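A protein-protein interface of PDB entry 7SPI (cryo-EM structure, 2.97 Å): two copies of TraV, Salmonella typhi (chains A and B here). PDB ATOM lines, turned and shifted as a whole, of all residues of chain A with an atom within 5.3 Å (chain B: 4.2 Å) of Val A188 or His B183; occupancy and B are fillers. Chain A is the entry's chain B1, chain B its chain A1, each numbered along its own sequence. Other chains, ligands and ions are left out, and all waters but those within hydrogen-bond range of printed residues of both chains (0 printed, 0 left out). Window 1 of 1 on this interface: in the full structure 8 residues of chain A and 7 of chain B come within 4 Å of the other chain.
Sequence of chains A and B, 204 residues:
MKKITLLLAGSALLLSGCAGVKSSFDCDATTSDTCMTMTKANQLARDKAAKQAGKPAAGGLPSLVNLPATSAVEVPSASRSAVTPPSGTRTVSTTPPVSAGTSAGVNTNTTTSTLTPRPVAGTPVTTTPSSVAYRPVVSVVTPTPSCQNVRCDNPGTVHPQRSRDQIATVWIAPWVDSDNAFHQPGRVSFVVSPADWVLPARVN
N of Phe B182 is in hydrogen-bond range of O of Ser A189 (2.8 Å).
O of Trp B175 sits at hydrogen-bond distance from N of His B183 (2.8 Å).
N of Ala B181 sits at hydrogen-bond distance from OD1 of Asp B177, 3.1 Å away.
The backbone carbonyl oxygen (O) of Ala B181 lies close to a ring nitrogen (NE2) of His B183 (3.3 Å).
The backbone carbonyl oxygen (O) of Phe A190 sits at hydrogen-bond distance from the backbone NH (N) of Ala A168 (3.1 Å).
The side-chain hydroxyl (OG1) of Thr A169 lies within hydrogen-bond range of the guanidinium group (NH1) of Arg A187.
The backbone carbonyl oxygen (O) of Val A170 sits at hydrogen-bond distance from the backbone NH (N) of Val A188 (3.1 Å).
Among the printed residues, merely in contact across the chains: Arg A187 with Gln B184 (3.3 Å), Val A188 with Ala B181 (3.4 Å), Val A188 with Phe B182 (2.9 Å), Val A188 with His B183 (3.9 Å), Ser A189 with Ala B181 (3.8 Å) and Phe A190 with Ala B181 (3.7 Å).
Thr A169 touches none of the printed residues of chain B.
Printed residues of chain B within 4 Å of Arg A187: Gln B184 (3.3 Å).
Of chain B, only Ala B181, Phe B182 and His B183 come within 4 Å of Val A188.
Of the printed residues of chain B, Ser A189 touches Ala B181 (3.8 Å) and Phe B182 (2.8 Å).
Trp B175 touches none of the printed residues of chain A.
His B183 touches one residue of chain A.
Of the printed residues of chain A, Gln B184 touches Arg A187 (3.3 Å).
The nearest printed residue of chain B that does not touch Val A188 is Gln B184 (5.2 Å).
The nearest residue of chain A that does not touch His B183 is Arg A187 (4.5 Å).
Of the 9 printed residues of chain A, 4 touch a printed residue of chain B.
Hydrophobic or aromatic side chains of chain A within 4 Å of the printed part of chain B: Val A188 and Phe A190.
Among the printed residues, no Asp or Glu carboxylate lies within 4 Å of a Lys or Arg side-chain nitrogen of the other chain.
No position is printed for both chains.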
ATOM      1  N   ALA A 168      -8.479 -24.669  26.064  1.00  0.00           N
ATOM      2  CA  ALA A 168      -9.120 -23.369  26.187  1.00  0.00           C
ATOM      3  C   ALA A 168     -10.563 -23.466  25.717  1.00  0.00           C
ATOM      4  O   ALA A 168     -10.875 -24.186  24.763  1.00  0.00           O
ATOM      5  CB  ALA A 168      -8.379 -22.295  25.383  1.00  0.00           C
ATOM      6  N   THR A 169     -11.441 -22.730  26.392  1.00  0.00           N
ATOM      7  CA  THR A 169     -12.866 -22.731  26.098  1.00  0.00           C
ATOM      8  C   THR A 169     -13.272 -21.397  25.492  1.00  0.00           C
ATOM      9  O   THR A 169     -12.831 -20.336  25.947  1.00  0.00           O
ATOM     10  CB  THR A 169     -13.696 -23.001  27.357  1.00  0.00           C
ATOM     11  OG1 THR A 169     -13.678 -21.842  28.199  1.00  0.00           O
ATOM     12  CG2 THR A 169     -13.128 -24.187  28.123  1.00  0.00           C
ATOM     13  N   VAL A 170     -14.119 -21.449  24.464  1.00  0.00           N
ATOM     14  CA  VAL A 170     -14.621 -20.240  23.813  1.00  0.00           C
ATOM     15  C   VAL A 170     -16.138 -20.291  23.897  1.00  0.00           C
ATOM     16  O   VAL A 170     -16.714 -21.373  23.881  1.00  0.00           O
ATOM     17  CB  VAL A 170     -14.187 -20.184  22.335  1.00  0.00           C
ATOM     18  CG1 VAL A 170     -14.735 -18.950  21.635  1.00  0.00           C
ATOM     19  CG2 VAL A 170     -12.673 -20.198  22.230  1.00  0.00           C
ATOM     20  N   ILE A 172     -19.671 -19.158  22.072  1.00  0.00           N
ATOM     21  CA  ILE A 172     -20.204 -18.643  20.825  1.00  0.00           C
ATOM     22  C   ILE A 172     -21.568 -18.016  21.055  1.00  0.00           C
ATOM     23  O   ILE A 172     -22.455 -18.657  21.610  1.00  0.00           O
ATOM     24  CB  ILE A 172     -20.295 -19.735  19.750  1.00  0.00           C
ATOM     25  CG1 ILE A 172     -18.986 -20.522  19.668  1.00  0.00           C
ATOM     26  CG2 ILE A 172     -20.634 -19.130  18.397  1.00  0.00           C
ATOM     27  CD1 ILE A 172     -17.852 -19.752  19.031  1.00  0.00           C
ATOM     28  N   GLY A 186     -23.086 -24.052  22.656  1.00  0.00           N
ATOM     29  CA  GLY A 186     -22.460 -24.107  23.968  1.00  0.00           C
ATOM     30  C   GLY A 186     -20.956 -23.979  23.873  1.00  0.00           C
ATOM     31  O   GLY A 186     -20.389 -24.137  22.792  1.00  0.00           O
ATOM     32  N   ARG A 187     -20.316 -23.669  24.998  1.00  0.00           N
ATOM     33  CA  ARG A 187     -18.869 -23.481  25.007  1.00  0.00           C
ATOM     34  C   ARG A 187     -18.131 -24.703  24.505  1.00  0.00           C
ATOM     35  O   ARG A 187     -18.443 -25.832  24.886  1.00  0.00           O
ATOM     36  CB  ARG A 187     -18.371 -23.112  26.406  1.00  0.00           C
ATOM     37  CG  ARG A 187     -18.895 -21.782  26.916  1.00  0.00           C
ATOM     38  CD  ARG A 187     -17.885 -21.118  27.836  1.00  0.00           C
ATOM     39  NE  ARG A 187     -17.487 -21.994  28.932  1.00  0.00           N
ATOM     40  CZ  ARG A 187     -16.597 -21.665  29.863  1.00  0.00           C
ATOM     41  NH1 ARG A 187     -16.008 -20.478  29.827  1.00  0.00           N
ATOM     42  NH2 ARG A 187     -16.293 -22.524  30.826  1.00  0.00           N
ATOM     43  N   VAL A 188     -17.138 -24.478  23.656  1.00  0.00           N
ATOM     44  CA  VAL A 188     -16.372 -25.589  23.118  1.00  0.00           C
ATOM     45  C   VAL A 188     -14.992 -25.614  23.758  1.00  0.00           C
ATOM     46  O   VAL A 188     -14.272 -24.615  23.750  1.00  0.00           O
ATOM     47  CB  VAL A 188     -16.286 -25.512  21.576  1.00  0.00           C
ATOM     48  CG1 VAL A 188     -16.015 -24.088  21.107  1.00  0.00           C
ATOM     49  CG2 VAL A 188     -15.265 -26.496  21.025  1.00  0.00           C
ATOM     50  N   SER A 189     -14.629 -26.754  24.332  1.00  0.00           N
ATOM     51  CA  SER A 189     -13.317 -26.877  24.946  1.00  0.00           C
ATOM     52  C   SER A 189     -12.450 -27.702  24.025  1.00  0.00           C
ATOM     53  O   SER A 189     -12.798 -28.832  23.680  1.00  0.00           O
ATOM     54  CB  SER A 189     -13.424 -27.540  26.319  1.00  0.00           C
ATOM     55  OG  SER A 189     -14.115 -28.774  26.240  1.00  0.00           O
ATOM     56  N   PHE A 190     -11.322 -27.141  23.615  1.00  0.00           N
ATOM     57  CA  PHE A 190     -10.456 -27.837  22.676  1.00  0.00           C
ATOM     58  C   PHE A 190      -9.005 -27.714  23.090  1.00  0.00           C
ATOM     59  O   PHE A 190      -8.617 -26.734  23.725  1.00  0.00           O
ATOM     60  CB  PHE A 190     -10.656 -27.293  21.255  1.00  0.00           C
ATOM     61  CG  PHE A 190     -10.618 -25.791  21.164  1.00  0.00           C
ATOM     62  CD1 PHE A 190     -11.779 -25.044  21.289  1.00  0.00           C
ATOM     63  CD2 PHE A 190      -9.423 -25.126  20.940  1.00  0.00           C
ATOM     64  CE1 PHE A 190     -11.747 -23.668  21.208  1.00  0.00           C
ATOM     65  CE2 PHE A 190      -9.385 -23.749  20.857  1.00  0.00           C
ATOM     66  CZ  PHE A 190     -10.549 -23.018  20.990  1.00  0.00           C
ATOM     67  N   PRO B 174     -23.590 -33.495  24.521  1.00  0.00           N
ATOM     68  CA  PRO B 174     -22.191 -33.210  24.199  1.00  0.00           C
ATOM     69  C   PRO B 174     -21.542 -34.083  23.135  1.00  0.00           C
ATOM     70  O   PRO B 174     -21.785 -35.288  23.107  1.00  0.00           O
ATOM     71  CB  PRO B 174     -21.473 -33.368  25.541  1.00  0.00           C
ATOM     72  CG  PRO B 174     -22.413 -34.114  26.415  1.00  0.00           C
ATOM     73  CD  PRO B 174     -23.753 -33.647  25.986  1.00  0.00           C
ATOM     74  N   TRP B 175     -20.710 -33.480  22.286  1.00  0.00           N
ATOM     75  CA  TRP B 175     -20.093 -34.230  21.196  1.00  0.00           C
ATOM     76  C   TRP B 175     -18.740 -33.719  20.724  1.00  0.00           C
ATOM     77  O   TRP B 175     -18.451 -32.536  20.831  1.00  0.00           O
ATOM     78  CB  TRP B 175     -21.056 -34.330  20.004  1.00  0.00           C
ATOM     79  CG  TRP B 175     -21.487 -33.008  19.435  1.00  0.00           C
ATOM     80  CD1 TRP B 175     -22.406 -32.147  19.960  1.00  0.00           C
ATOM     81  CD2 TRP B 175     -21.031 -32.411  18.216  1.00  0.00           C
ATOM     82  NE1 TRP B 175     -22.542 -31.046  19.152  1.00  0.00           N
ATOM     83  CE2 TRP B 175     -21.710 -31.183  18.074  1.00  0.00           C
ATOM     84  CE3 TRP B 175     -20.113 -32.790  17.235  1.00  0.00           C
ATOM     85  CZ2 TRP B 175     -21.498 -30.335  16.991  1.00  0.00           C
ATOM     86  CZ3 TRP B 175     -19.907 -31.949  16.160  1.00  0.00           C
ATOM     87  CH2 TRP B 175     -20.594 -30.735  16.047  1.00  0.00           C
ATOM     88  N   ASP B 177     -16.214 -33.413  17.422  1.00  0.00           N
ATOM     89  CA  ASP B 177     -16.218 -33.397  15.967  1.00  0.00           C
ATOM     90  C   ASP B 177     -14.911 -33.974  15.426  1.00  0.00           C
ATOM     91  O   ASP B 177     -14.093 -34.537  16.155  1.00  0.00           O
ATOM     92  CB  ASP B 177     -16.445 -31.980  15.446  1.00  0.00           C
ATOM     93  CG  ASP B 177     -15.508 -30.973  16.075  1.00  0.00           C
ATOM     94  OD1 ASP B 177     -15.364 -30.991  17.312  1.00  0.00           O
ATOM     95  OD2 ASP B 177     -14.918 -30.162  15.329  1.00  0.00           O
ATOM     96  N   ALA B 181     -12.760 -30.943  19.057  1.00  0.00           N
ATOM     97  CA  ALA B 181     -13.124 -29.867  19.959  1.00  0.00           C
ATOM     98  C   ALA B 181     -14.402 -30.334  20.619  1.00  0.00           C
ATOM     99  O   ALA B 181     -15.354 -30.687  19.937  1.00  0.00           O
ATOM    100  CB  ALA B 181     -13.364 -28.593  19.181  1.00  0.00           C
ATOM    101  N   PHE B 182     -14.421 -30.327  21.948  1.00  0.00           N
ATOM    102  CA  PHE B 182     -15.595 -30.762  22.699  1.00  0.00           C
ATOM    103  C   PHE B 182     -16.738 -29.767  22.540  1.00  0.00           C
ATOM    104  O   PHE B 182     -16.522 -28.558  22.606  1.00  0.00           O
ATOM    105  CB  PHE B 182     -15.218 -30.883  24.176  1.00  0.00           C
ATOM    106  CG  PHE B 182     -16.120 -31.779  24.970  1.00  0.00           C
ATOM    107  CD1 PHE B 182     -15.830 -33.126  25.104  1.00  0.00           C
ATOM    108  CD2 PHE B 182     -17.245 -31.276  25.599  1.00  0.00           C
ATOM    109  CE1 PHE B 182     -16.651 -33.956  25.840  1.00  0.00           C
ATOM    110  CE2 PHE B 182     -18.072 -32.101  26.334  1.00  0.00           C
ATOM    111  CZ  PHE B 182     -17.773 -33.443  26.455  1.00  0.00           C
ATOM    112  N   HIS B 183     -17.952 -30.267  22.333  1.00  0.00           N
ATOM    113  CA  HIS B 183     -19.112 -29.387  22.218  1.00  0.00           C
ATOM    114  C   HIS B 183     -20.121 -29.683  23.310  1.00  0.00           C
ATOM    115  O   HIS B 183     -20.859 -30.650  23.207  1.00  0.00           O
ATOM    116  CB  HIS B 183     -19.769 -29.521  20.846  1.00  0.00           C
ATOM    117  CG  HIS B 183     -18.860 -29.184  19.708  1.00  0.00           C
ATOM    118  ND1 HIS B 183     -18.487 -27.891  19.412  1.00  0.00           N
ATOM    119  CD2 HIS B 183     -18.249 -29.970  18.792  1.00  0.00           C
ATOM    120  CE1 HIS B 183     -17.684 -27.896  18.364  1.00  0.00           C
ATOM    121  NE2 HIS B 183     -17.524 -29.145  17.968  1.00  0.00           N
ATOM    122  N   GLN B 184     -20.174 -28.844  24.339  1.00  0.00           N
ATOM    123  CA  GLN B 184     -21.079 -29.039  25.469  1.00  0.00           C
ATOM    124  C   GLN B 184     -22.538 -28.968  25.023  1.00  0.00           C
ATOM    125  O   GLN B 184     -22.836 -28.431  23.956  1.00  0.00           O
ATOM    126  CB  GLN B 184     -20.795 -27.979  26.538  1.00  0.00           C
ATOM    127  CG  GLN B 184     -19.403 -28.060  27.138  1.00  0.00           C
ATOM    128  CD  GLN B 184     -19.286 -27.266  28.422  1.00  0.00           C
ATOM    129  OE1 GLN B 184     -20.290 -26.886  29.024  1.00  0.00           O
ATOM    130  NE2 GLN B 184     -18.055 -27.019  28.855  1.00  0.00           N
ATOM    131  N   PRO B 185     -23.466 -29.527  25.860  1.00  0.00           N
ATOM    132  CA  PRO B 185     -24.848 -29.543  25.366  1.00  0.00           C
ATOM    133  C   PRO B 185     -25.467 -28.214  25.003  1.00  0.00           C
ATOM    134  O   PRO B 185     -25.367 -27.249  25.761  1.00  0.00           O
ATOM    135  CB  PRO B 185     -25.641 -30.186  26.511  1.00  0.00           C
ATOM    136  CG  PRO B 185     -24.751 -30.186  27.686  1.00  0.00           C
ATOM    137  CD  PRO B 185     -23.370 -30.258  27.148  1.00  0.00           C
